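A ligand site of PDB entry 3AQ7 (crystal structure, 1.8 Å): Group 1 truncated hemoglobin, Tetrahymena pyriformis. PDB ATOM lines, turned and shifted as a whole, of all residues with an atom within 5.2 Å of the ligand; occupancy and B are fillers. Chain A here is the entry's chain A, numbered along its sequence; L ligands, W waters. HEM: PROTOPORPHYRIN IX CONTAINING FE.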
ATOM      1  N   VAL A  34     -18.951  22.664 -20.316  1.00  0.00           N
ATOM      2  CA  VAL A  34     -17.602  23.048 -20.600  1.00  0.00           C
ATOM      3  C   VAL A  34     -17.281  24.569 -20.583  1.00  0.00           C
ATOM      4  O   VAL A  34     -16.097  24.950 -20.683  1.00  0.00           O
ATOM      5  CB  VAL A  34     -17.131  22.561 -22.010  1.00  0.00           C
ATOM      6  CG1 VAL A  34     -16.886  20.987 -21.973  1.00  0.00           C
ATOM      7  CG2 VAL A  34     -18.136  22.881 -23.105  1.00  0.00           C
ATOM      8  N   PHE A  37     -14.390  26.255 -18.348  1.00  0.00           N
ATOM      9  CA  PHE A  37     -12.966  26.049 -18.616  1.00  0.00           C
ATOM     10  C   PHE A  37     -12.315  27.284 -19.302  1.00  0.00           C
ATOM     11  O   PHE A  37     -11.100  27.473 -19.211  1.00  0.00           O
ATOM     12  CB  PHE A  37     -12.727  24.791 -19.497  1.00  0.00           C
ATOM     13  CG  PHE A  37     -12.996  23.519 -18.713  1.00  0.00           C
ATOM     14  CD1 PHE A  37     -14.187  22.844 -18.888  1.00  0.00           C
ATOM     15  CD2 PHE A  37     -12.103  23.110 -17.731  1.00  0.00           C
ATOM     16  CE1 PHE A  37     -14.464  21.690 -18.108  1.00  0.00           C
ATOM     17  CE2 PHE A  37     -12.357  22.017 -16.968  1.00  0.00           C
ATOM     18  CZ  PHE A  37     -13.546  21.328 -17.146  1.00  0.00           C
ATOM     19  N   PHE A  38     -13.170  28.071 -19.972  1.00  0.00           N
ATOM     20  CA  PHE A  38     -12.777  29.275 -20.663  1.00  0.00           C
ATOM     21  C   PHE A  38     -12.846  30.563 -19.924  1.00  0.00           C
ATOM     22  O   PHE A  38     -12.543  31.637 -20.548  1.00  0.00           O
ATOM     23  CB  PHE A  38     -13.591  29.295 -22.011  1.00  0.00           C
ATOM     24  CG  PHE A  38     -13.326  28.060 -22.850  1.00  0.00           C
ATOM     25  CD1 PHE A  38     -14.186  26.918 -22.789  1.00  0.00           C
ATOM     26  CD2 PHE A  38     -12.119  27.991 -23.604  1.00  0.00           C
ATOM     27  CE1 PHE A  38     -13.879  25.763 -23.504  1.00  0.00           C
ATOM     28  CE2 PHE A  38     -11.799  26.747 -24.311  1.00  0.00           C
ATOM     29  CZ  PHE A  38     -12.703  25.698 -24.211  1.00  0.00           C
ATOM     30  N   ASN A  40     -10.933  32.284 -17.971  1.00  0.00           N
ATOM     31  CA  ASN A  40      -9.824  33.234 -17.942  1.00  0.00           C
ATOM     32  C   ASN A  40      -9.092  33.181 -19.273  1.00  0.00           C
ATOM     33  O   ASN A  40      -7.942  33.634 -19.357  1.00  0.00           O
ATOM     34  CB  ASN A  40      -8.823  32.895 -16.834  1.00  0.00           C
ATOM     35  CG  ASN A  40      -9.437  32.981 -15.463  1.00  0.00           C
ATOM     36  OD1 ASN A  40     -10.090  33.981 -15.143  1.00  0.00           O
ATOM     37  ND2 ASN A  40      -9.263  31.934 -14.637  1.00  0.00           N
ATOM     38  N   THR A  41      -9.743  32.698 -20.335  1.00  0.00           N
ATOM     39  CA  THR A  41      -9.088  32.531 -21.622  1.00  0.00           C
ATOM     40  C   THR A  41      -9.148  33.753 -22.499  1.00  0.00           C
ATOM     41  O   THR A  41     -10.181  34.434 -22.536  1.00  0.00           O
ATOM     42  CB  THR A  41      -9.692  31.340 -22.375  1.00  0.00           C
ATOM     43  OG1 THR A  41      -9.330  30.159 -21.647  1.00  0.00           O
ATOM     44  CG2 THR A  41      -9.075  31.181 -23.807  1.00  0.00           C
ATOM     45  N   ASP A  42      -8.022  34.096 -23.131  1.00  0.00           N
ATOM     46  CA  ASP A  42      -8.036  35.233 -24.076  1.00  0.00           C
ATOM     47  C   ASP A  42      -8.733  34.644 -25.341  1.00  0.00           C
ATOM     48  O   ASP A  42      -8.101  33.881 -26.111  1.00  0.00           O
ATOM     49  CB  ASP A  42      -6.585  35.688 -24.308  1.00  0.00           C
ATOM     50  CG  ASP A  42      -6.423  36.591 -25.548  1.00  0.00           C
ATOM     51  OD1 ASP A  42      -7.378  36.757 -26.381  1.00  0.00           O
ATOM     52  OD2 ASP A  42      -5.305  37.151 -25.698  1.00  0.00           O
ATOM     53  N   HIS A  45      -7.060  35.296 -28.987  1.00  0.00           N
ATOM     54  CA  HIS A  45      -5.945  34.366 -29.167  1.00  0.00           C
ATOM     55  C   HIS A  45      -6.377  32.932 -29.375  1.00  0.00           C
ATOM     56  O   HIS A  45      -5.831  32.185 -30.266  1.00  0.00           O
ATOM     57  CB  HIS A  45      -4.908  34.432 -28.026  1.00  0.00           C
ATOM     58  CG  HIS A  45      -3.668  33.604 -28.283  1.00  0.00           C
ATOM     59  ND1 HIS A  45      -3.406  32.410 -27.633  1.00  0.00           N
ATOM     60  CD2 HIS A  45      -2.649  33.796 -29.154  1.00  0.00           C
ATOM     61  CE1 HIS A  45      -2.257  31.907 -28.067  1.00  0.00           C
ATOM     62  NE2 HIS A  45      -1.773  32.726 -28.984  1.00  0.00           N
ATOM     63  N   GLN A  46      -7.325  32.466 -28.572  1.00  0.00           N
ATOM     64  CA  GLN A  46      -7.782  31.107 -28.682  1.00  0.00           C
ATOM     65  C   GLN A  46      -8.518  30.950 -30.066  1.00  0.00           C
ATOM     66  O   GLN A  46      -8.498  29.826 -30.667  1.00  0.00           O
ATOM     67  CB  GLN A  46      -8.596  30.747 -27.447  1.00  0.00           C
ATOM     68  CG  GLN A  46      -9.593  29.525 -27.550  1.00  0.00           C
ATOM     69  CD  GLN A  46      -8.815  28.198 -27.515  1.00  0.00           C
ATOM     70  OE1 GLN A  46      -7.549  28.237 -27.236  1.00  0.00           O
ATOM     71  NE2 GLN A  46      -9.501  27.037 -27.840  1.00  0.00           N
ATOM     72  N   GLN A  49      -5.651  30.306 -32.555  1.00  0.00           N
ATOM     73  CA  GLN A  49      -5.044  28.994 -32.384  1.00  0.00           C
ATOM     74  C   GLN A  49      -5.942  27.912 -32.848  1.00  0.00           C
ATOM     75  O   GLN A  49      -5.461  26.948 -33.486  1.00  0.00           O
ATOM     76  CB  GLN A  49      -4.635  28.720 -30.908  1.00  0.00           C
ATOM     77  CG  GLN A  49      -3.509  29.691 -30.489  1.00  0.00           C
ATOM     78  CD  GLN A  49      -2.316  29.604 -31.445  1.00  0.00           C
ATOM     79  OE1 GLN A  49      -1.799  28.553 -31.721  1.00  0.00           O
ATOM     80  NE2 GLN A  49      -1.944  30.687 -31.997  1.00  0.00           N
ATOM     81  N   GLN A  50      -7.225  27.987 -32.483  1.00  0.00           N
ATOM     82  CA  GLN A  50      -8.125  26.903 -32.826  1.00  0.00           C
ATOM     83  C   GLN A  50      -8.401  26.905 -34.329  1.00  0.00           C
ATOM     84  O   GLN A  50      -8.504  25.825 -34.961  1.00  0.00           O
ATOM     85  CB  GLN A  50      -9.450  27.172 -32.094  1.00  0.00           C
ATOM     86  CG  GLN A  50     -10.417  26.077 -32.293  1.00  0.00           C
ATOM     87  CD  GLN A  50     -10.109  24.817 -31.437  1.00  0.00           C
ATOM     88  OE1 GLN A  50      -9.675  24.882 -30.253  1.00  0.00           O
ATOM     89  NE2 GLN A  50     -10.304  23.706 -32.040  1.00  0.00           N
ATOM     90  N   PHE A  53      -5.380  25.299 -35.819  1.00  0.00           N
ATOM     91  CA  PHE A  53      -5.276  23.857 -35.496  1.00  0.00           C
ATOM     92  C   PHE A  53      -6.258  23.016 -36.322  1.00  0.00           C
ATOM     93  O   PHE A  53      -5.887  22.012 -36.972  1.00  0.00           O
ATOM     94  CB  PHE A  53      -5.581  23.644 -33.983  1.00  0.00           C
ATOM     95  CG  PHE A  53      -5.286  22.182 -33.593  1.00  0.00           C
ATOM     96  CD1 PHE A  53      -3.994  21.737 -33.600  1.00  0.00           C
ATOM     97  CD2 PHE A  53      -6.294  21.361 -33.213  1.00  0.00           C
ATOM     98  CE1 PHE A  53      -3.630  20.448 -33.232  1.00  0.00           C
ATOM     99  CE2 PHE A  53      -5.985  20.046 -32.834  1.00  0.00           C
ATOM    100  CZ  PHE A  53      -4.608  19.592 -32.808  1.00  0.00           C
ATOM    101  N   LEU A  54      -7.542  23.455 -36.371  1.00  0.00           N
ATOM    102  CA  LEU A  54      -8.503  22.755 -37.182  1.00  0.00           C
ATOM    103  C   LEU A  54      -8.174  22.829 -38.654  1.00  0.00           C
ATOM    104  O   LEU A  54      -8.351  21.878 -39.410  1.00  0.00           O
ATOM    105  CB  LEU A  54      -9.935  23.224 -36.904  1.00  0.00           C
ATOM    106  CG  LEU A  54     -10.367  22.952 -35.449  1.00  0.00           C
ATOM    107  CD1 LEU A  54     -11.729  23.719 -35.273  1.00  0.00           C
ATOM    108  CD2 LEU A  54     -10.392  21.469 -35.088  1.00  0.00           C
ATOM    109  N   LEU A  57      -5.500  20.306 -39.153  1.00  0.00           N
ATOM    110  CA  LEU A  57      -5.909  18.876 -38.923  1.00  0.00           C
ATOM    111  C   LEU A  57      -6.784  18.346 -40.078  1.00  0.00           C
ATOM    112  O   LEU A  57      -6.722  17.156 -40.450  1.00  0.00           O
ATOM    113  CB  LEU A  57      -6.838  18.790 -37.711  1.00  0.00           C
ATOM    114  CG  LEU A  57      -6.581  17.618 -36.800  1.00  0.00           C
ATOM    115  CD1 LEU A  57      -5.003  17.294 -36.386  1.00  0.00           C
ATOM    116  CD2 LEU A  57      -7.146  18.068 -35.512  1.00  0.00           C
ATOM    117  N   TYR A  64      -0.119  25.938 -37.976  1.00  0.00           N
ATOM    118  CA  TYR A  64      -0.375  25.803 -36.530  1.00  0.00           C
ATOM    119  C   TYR A  64       0.946  25.824 -35.790  1.00  0.00           C
ATOM    120  O   TYR A  64       1.840  24.931 -36.010  1.00  0.00           O
ATOM    121  CB  TYR A  64      -1.128  24.526 -36.212  1.00  0.00           C
ATOM    122  CG  TYR A  64      -1.366  24.337 -34.746  1.00  0.00           C
ATOM    123  CD1 TYR A  64      -2.202  25.261 -34.086  1.00  0.00           C
ATOM    124  CD2 TYR A  64      -0.713  23.363 -34.009  1.00  0.00           C
ATOM    125  CE1 TYR A  64      -2.427  25.175 -32.722  1.00  0.00           C
ATOM    126  CE2 TYR A  64      -0.935  23.240 -32.586  1.00  0.00           C
ATOM    127  CZ  TYR A  64      -1.791  24.207 -31.964  1.00  0.00           C
ATOM    128  OH  TYR A  64      -1.965  24.068 -30.619  1.00  0.00           O
ATOM    129  N   GLY A  66       0.935  26.284 -32.328  1.00  0.00           N
ATOM    130  CA  GLY A  66       0.661  26.156 -30.861  1.00  0.00           C
ATOM    131  C   GLY A  66       1.127  24.886 -30.144  1.00  0.00           C
ATOM    132  O   GLY A  66       1.857  24.041 -30.727  1.00  0.00           O
ATOM    133  N   LYS A  67       0.626  24.672 -28.912  1.00  0.00           N
ATOM    134  CA  LYS A  67       1.021  23.587 -28.129  1.00  0.00           C
ATOM    135  C   LYS A  67       0.405  22.278 -28.663  1.00  0.00           C
ATOM    136  O   LYS A  67      -0.601  22.279 -29.349  1.00  0.00           O
ATOM    137  CB  LYS A  67       0.443  23.742 -26.710  1.00  0.00           C
ATOM    138  CG  LYS A  67       1.195  24.866 -25.939  1.00  0.00           C
ATOM    139  CD  LYS A  67       0.391  25.237 -24.627  1.00  0.00           C
ATOM    140  CE  LYS A  67       1.014  26.494 -23.858  1.00  0.00           C
ATOM    141  NZ  LYS A  67       0.720  26.267 -22.397  1.00  0.00           N
ATOM    142  N   MET A  69      -1.626  18.577 -27.947  1.00  0.00           N
ATOM    143  CA  MET A  69      -2.901  18.498 -27.270  1.00  0.00           C
ATOM    144  C   MET A  69      -2.720  18.032 -25.840  1.00  0.00           C
ATOM    145  O   MET A  69      -3.586  18.266 -24.996  1.00  0.00           O
ATOM    146  CB  MET A  69      -3.879  17.575 -28.031  1.00  0.00           C
ATOM    147  CG  MET A  69      -4.364  18.158 -29.377  1.00  0.00           C
ATOM    148  SD  MET A  69      -5.255  19.738 -29.147  1.00  0.00           S
ATOM    149  CE  MET A  69      -3.979  21.005 -29.373  1.00  0.00           C
ATOM    150  N   ALA A  72      -1.510  21.536 -24.197  1.00  0.00           N
ATOM    151  CA  ALA A  72      -2.602  22.503 -24.234  1.00  0.00           C
ATOM    152  C   ALA A  72      -3.587  22.293 -23.068  1.00  0.00           C
ATOM    153  O   ALA A  72      -4.052  23.268 -22.486  1.00  0.00           O
ATOM    154  CB  ALA A  72      -3.314  22.424 -25.527  1.00  0.00           C
ATOM    155  N   HIS A  73      -3.769  21.058 -22.626  1.00  0.00           N
ATOM    156  CA  HIS A  73      -4.804  20.738 -21.648  1.00  0.00           C
ATOM    157  C   HIS A  73      -4.199  20.196 -20.375  1.00  0.00           C
ATOM    158  O   HIS A  73      -4.930  19.556 -19.552  1.00  0.00           O
ATOM    159  CB  HIS A  73      -5.858  19.749 -22.265  1.00  0.00           C
ATOM    160  CG  HIS A  73      -6.452  20.310 -23.516  1.00  0.00           C
ATOM    161  ND1 HIS A  73      -5.975  19.992 -24.773  1.00  0.00           N
ATOM    162  CD2 HIS A  73      -7.363  21.291 -23.709  1.00  0.00           C
ATOM    163  CE1 HIS A  73      -6.675  20.621 -25.700  1.00  0.00           C
ATOM    164  NE2 HIS A  73      -7.487  21.462 -25.072  1.00  0.00           N
ATOM    165  N   MET A  76      -5.709  20.137 -16.469  1.00  0.00           N
ATOM    166  CA  MET A  76      -7.179  20.322 -16.492  1.00  0.00           C
ATOM    167  C   MET A  76      -7.908  19.001 -16.078  1.00  0.00           C
ATOM    168  O   MET A  76      -8.996  19.056 -15.587  1.00  0.00           O
ATOM    169  CB  MET A  76      -7.622  20.737 -17.877  1.00  0.00           C
ATOM    170  CG  MET A  76      -7.101  22.169 -18.297  1.00  0.00           C
ATOM    171  SD  MET A  76      -7.711  22.489 -19.893  1.00  0.00           S
ATOM    172  CE  MET A  76      -6.733  23.956 -20.269  1.00  0.00           C
ATOM    173  N   LEU A  78      -9.129  16.687 -17.830  1.00  0.00           N
ATOM    174  CA  LEU A  78     -10.357  16.647 -18.602  1.00  0.00           C
ATOM    175  C   LEU A  78     -10.941  15.210 -18.614  1.00  0.00           C
ATOM    176  O   LEU A  78     -10.174  14.211 -18.600  1.00  0.00           O
ATOM    177  CB  LEU A  78     -10.086  17.048 -20.065  1.00  0.00           C
ATOM    178  CG  LEU A  78     -10.335  18.520 -20.347  1.00  0.00           C
ATOM    179  CD1 LEU A  78     -10.564  19.415 -19.400  1.00  0.00           C
ATOM    180  CD2 LEU A  78      -9.304  18.999 -21.487  1.00  0.00           C
ATOM    181  N   HIS A  82     -16.409  15.909 -21.166  1.00  0.00           N
ATOM    182  CA  HIS A  82     -15.975  17.247 -21.685  1.00  0.00           C
ATOM    183  C   HIS A  82     -15.646  17.093 -23.166  1.00  0.00           C
ATOM    184  O   HIS A  82     -16.061  17.930 -23.978  1.00  0.00           O
ATOM    185  CB  HIS A  82     -14.735  17.728 -20.948  1.00  0.00           C
ATOM    186  CG  HIS A  82     -14.956  17.878 -19.462  1.00  0.00           C
ATOM    187  ND1 HIS A  82     -15.970  18.648 -18.901  1.00  0.00           N
ATOM    188  CD2 HIS A  82     -14.234  17.402 -18.420  1.00  0.00           C
ATOM    189  CE1 HIS A  82     -15.883  18.609 -17.560  1.00  0.00           C
ATOM    190  NE2 HIS A  82     -14.838  17.884 -17.258  1.00  0.00           N
ATOM    191  N   PHE A  83     -14.956  16.005 -23.552  1.00  0.00           N
ATOM    192  CA  PHE A  83     -14.626  15.839 -24.953  1.00  0.00           C
ATOM    193  C   PHE A  83     -15.863  15.563 -25.822  1.00  0.00           C
ATOM    194  O   PHE A  83     -15.980  16.204 -26.905  1.00  0.00           O
ATOM    195  CB  PHE A  83     -13.547  14.718 -25.079  1.00  0.00           C
ATOM    196  CG  PHE A  83     -12.962  14.611 -26.505  1.00  0.00           C
ATOM    197  CD1 PHE A  83     -11.735  15.195 -26.788  1.00  0.00           C
ATOM    198  CD2 PHE A  83     -13.639  13.912 -27.498  1.00  0.00           C
ATOM    199  CE1 PHE A  83     -11.169  15.128 -28.036  1.00  0.00           C
ATOM    200  CE2 PHE A  83     -13.087  13.787 -28.731  1.00  0.00           C
ATOM    201  CZ  PHE A  83     -11.843  14.416 -29.032  1.00  0.00           C
ATOM    202  N   ILE A  86     -17.396  18.944 -26.540  1.00  0.00           N
ATOM    203  CA  ILE A  86     -16.716  19.731 -27.596  1.00  0.00           C
ATOM    204  C   ILE A  86     -17.124  19.160 -28.958  1.00  0.00           C
ATOM    205  O   ILE A  86     -17.469  19.943 -29.884  1.00  0.00           O
ATOM    206  CB  ILE A  86     -15.199  19.694 -27.361  1.00  0.00           C
ATOM    207  CG1 ILE A  86     -14.853  20.378 -26.056  1.00  0.00           C
ATOM    208  CG2 ILE A  86     -14.417  20.300 -28.657  1.00  0.00           C
ATOM    209  CD1 ILE A  86     -15.337  21.833 -25.888  1.00  0.00           C
ATOM    210  N   ILE A 111     -10.761  14.386 -35.706  1.00  0.00           N
ATOM    211  CA  ILE A 111     -10.597  15.043 -34.390  1.00  0.00           C
ATOM    212  C   ILE A 111     -10.657  14.063 -33.241  1.00  0.00           C
ATOM    213  O   ILE A 111      -9.969  14.194 -32.253  1.00  0.00           O
ATOM    214  CB  ILE A 111     -11.702  16.146 -34.215  1.00  0.00           C
ATOM    215  CG1 ILE A 111     -11.439  17.159 -35.320  1.00  0.00           C
ATOM    216  CG2 ILE A 111     -11.652  16.749 -32.770  1.00  0.00           C
ATOM    217  CD1 ILE A 111     -12.615  18.092 -35.602  1.00  0.00           C
ATOM    218  N   THR A 114      -7.663  12.732 -31.219  1.00  0.00           N
ATOM    219  CA  THR A 114      -6.979  13.559 -30.202  1.00  0.00           C
ATOM    220  C   THR A 114      -7.470  13.283 -28.775  1.00  0.00           C
ATOM    221  O   THR A 114      -6.857  13.772 -27.821  1.00  0.00           O
ATOM    222  CB  THR A 114      -7.129  15.092 -30.448  1.00  0.00           C
ATOM    223  OG1 THR A 114      -8.508  15.545 -30.271  1.00  0.00           O
ATOM    224  CG2 THR A 114      -6.568  15.471 -31.792  1.00  0.00           C
ATOM    225  N   MET A 118      -5.571  14.333 -24.670  1.00  0.00           N
ATOM    226  CA  MET A 118      -5.909  15.479 -23.745  1.00  0.00           C
ATOM    227  C   MET A 118      -6.702  15.089 -22.493  1.00  0.00           C
ATOM    228  O   MET A 118      -6.794  15.869 -21.579  1.00  0.00           O
ATOM    229  CB  MET A 118      -6.674  16.575 -24.514  1.00  0.00           C
ATOM    230  CG  MET A 118      -7.998  16.080 -25.138  1.00  0.00           C
ATOM    231  SD  MET A 118      -8.848  17.435 -25.995  1.00  0.00           S
ATOM    232  CE  MET A 118      -7.891  17.525 -27.522  1.00  0.00           C
ATOM    233  N   LEU A 119      -7.325  13.890 -22.476  1.00  0.00           N
ATOM    234  CA  LEU A 119      -8.060  13.489 -21.258  1.00  0.00           C
ATOM    235  C   LEU A 119      -7.092  13.106 -20.119  1.00  0.00           C
ATOM    236  O   LEU A 119      -6.058  12.468 -20.336  1.00  0.00           O
ATOM    237  CB  LEU A 119      -8.960  12.266 -21.487  1.00  0.00           C
ATOM    238  CG  LEU A 119     -10.146  12.508 -22.491  1.00  0.00           C
ATOM    239  CD1 LEU A 119     -10.977  11.205 -22.389  1.00  0.00           C
ATOM    240  CD2 LEU A 119     -10.924  13.804 -22.171  1.00  0.00           C
HETATM  241  CHA HEM L   1      -6.279  25.172 -25.423  1.00  0.00           C
HETATM  242  CHB HEM L   1     -10.358  23.654 -23.163  1.00  0.00           C
HETATM  243  CHC HEM L   1     -10.884  19.981 -26.237  1.00  0.00           C
HETATM  244  CHD HEM L   1      -7.779  22.373 -29.128  1.00  0.00           C
HETATM  245  C1A HEM L   1      -7.296  25.049 -24.561  1.00  0.00           C
HETATM  246  C2A HEM L   1      -7.524  25.884 -23.325  1.00  0.00           C
HETATM  247  C3A HEM L   1      -8.666  25.490 -22.766  1.00  0.00           C
HETATM  248  C4A HEM L   1      -9.228  24.335 -23.487  1.00  0.00           C
HETATM  249  CMA HEM L   1      -9.275  26.094 -21.419  1.00  0.00           C
HETATM  250  CAA HEM L   1      -6.570  27.098 -23.106  1.00  0.00           C
HETATM  251  CBA HEM L   1      -6.003  27.608 -21.804  1.00  0.00           C
HETATM  252  CGA HEM L   1      -5.750  29.101 -22.215  1.00  0.00           C
HETATM  253  O1A HEM L   1      -4.788  29.339 -23.015  1.00  0.00           O
HETATM  254  O2A HEM L   1      -6.516  30.015 -21.841  1.00  0.00           O
HETATM  255  C1B HEM L   1     -10.750  22.494 -23.800  1.00  0.00           C
HETATM  256  C2B HEM L   1     -11.722  21.628 -23.191  1.00  0.00           C
HETATM  257  C3B HEM L   1     -11.830  20.563 -23.999  1.00  0.00           C
HETATM  258  C4B HEM L   1     -10.912  20.816 -25.090  1.00  0.00           C
HETATM  259  CMB HEM L   1     -12.546  21.785 -21.871  1.00  0.00           C
HETATM  260  CAB HEM L   1     -12.768  19.340 -23.736  1.00  0.00           C
HETATM  261  CBB HEM L   1     -12.153  18.197 -23.961  1.00  0.00           C
HETATM  262  C1C HEM L   1     -10.225  20.401 -27.353  1.00  0.00           C
HETATM  263  C2C HEM L   1     -10.216  19.805 -28.724  1.00  0.00           C
HETATM  264  C3C HEM L   1      -9.328  20.471 -29.483  1.00  0.00           C
HETATM  265  C4C HEM L   1      -8.712  21.540 -28.675  1.00  0.00           C
HETATM  266  CMC HEM L   1     -11.158  18.571 -29.002  1.00  0.00           C
HETATM  267  CAC HEM L   1      -8.935  20.312 -31.013  1.00  0.00           C
HETATM  268  CBC HEM L   1      -9.737  19.514 -31.621  1.00  0.00           C
HETATM  269  C1D HEM L   1      -7.115  23.284 -28.367  1.00  0.00           C
HETATM  270  C2D HEM L   1      -6.060  24.104 -28.941  1.00  0.00           C
HETATM  271  C3D HEM L   1      -5.610  24.976 -27.801  1.00  0.00           C
HETATM  272  C4D HEM L   1      -6.434  24.548 -26.712  1.00  0.00           C
HETATM  273  CMD HEM L   1      -5.508  24.247 -30.383  1.00  0.00           C
HETATM  274  CAD HEM L   1      -4.539  26.057 -27.877  1.00  0.00           C
HETATM  275  CBD HEM L   1      -3.139  25.653 -27.539  1.00  0.00           C
HETATM  276  CGD HEM L   1      -2.217  26.870 -27.701  1.00  0.00           C
HETATM  277  O1D HEM L   1      -1.044  26.702 -28.007  1.00  0.00           O
HETATM  278  O2D HEM L   1      -2.671  28.016 -27.290  1.00  0.00           O
HETATM  279  NA  HEM L   1      -8.328  24.218 -24.506  1.00  0.00           N
HETATM  280  NB  HEM L   1     -10.156  22.027 -25.031  1.00  0.00           N
HETATM  281  NC  HEM L   1      -9.334  21.362 -27.468  1.00  0.00           N
HETATM  282  ND  HEM L   1      -7.402  23.527 -26.971  1.00  0.00           N
HETATM  283 FE   HEM L   1      -8.782  22.771 -25.979  1.00  0.00          FE
HETATM  284  O   HOH W   1     -10.400  24.041 -26.903  1.00  0.00           O
HETATM  285  O   HOH W   2      -5.588  32.537 -23.047  1.00  0.00           O
HETATM  286  O   HOH W   3       0.694  28.719 -27.971  1.00  0.00           O
HETATM  287  O   HOH W   4      -5.256  29.628 -26.904  1.00  0.00           O
HETATM  288  O   HOH W   5      -3.442  27.845 -24.534  1.00  0.00           O
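The side-chain hydroxyl of Thr 41 is in hydrogen-bond range of an oxygen (O2A) of the ligand (2.8 Å). NE2 of His 73 binds FE of the ligand, 2.1 Å away. The backbone NH (N) of Lys 67 lies within hydrogen-bond range of an oxygen (O1D) of the ligand (2.8 Å).
The backbone NH (N) of His 45 lies within hydrogen-bond range of the side-chain carboxylate (OD1) of Asp 42 (3.0 Å). The side-chain amide oxygen of Gln 50 lies within hydrogen-bond range of the side-chain amide nitrogen of Gln 46 (3.2 Å). OG1 of Thr 114 lies within hydrogen-bond range of O of Ile 111, 2.8 Å away. A ring nitrogen (ND1) of His 73 is in hydrogen-bond range of the backbone carbonyl oxygen (O) of Met 69 (3.0 Å). OH of Tyr 64 is in hydrogen-bond range of O of Lys 67 (2.6 Å).
O of Phe 37 touches CMA of the ligand, 3.2 Å away. CZ of Phe 38 touches CHB of the ligand, at 3.3 Å. His 45 touches the ligand (CE1 to O2D, 3.99 Å). Gln 46 touches the ligand. Gln 49 touches the ligand. Gln 50 touches the ligand. Phe 53 touches the ligand (CE2 to CAC, 3.5 Å). Tyr 64 touches the ligand. Gly 66 touches the ligand. Met 69 touches the ligand (SD to CHD, 3.6 Å). Ala 72 touches the ligand. Met 76 touches the ligand. Leu 78 touches the ligand. His 82 touches the ligand (O to CAB, 3.6 Å). CA of Phe 83 touches CBB of the ligand (3.6 Å). CG1 of Ile 86 touches CAB of the ligand, at 3.3 Å. Ile 111 touches the ligand. Met 118 touches the ligand. The nearest printed residue that does not touch the ligand is Leu 54 (4.03 Å).
Water W2 lies within hydrogen-bond range of N of Asp 42 (2.9 Å) and O2A of the ligand (2.9 Å). Water W4 lies within hydrogen-bond range of OE1 of Gln 46, O2D of the ligand and ND1 of His 45.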
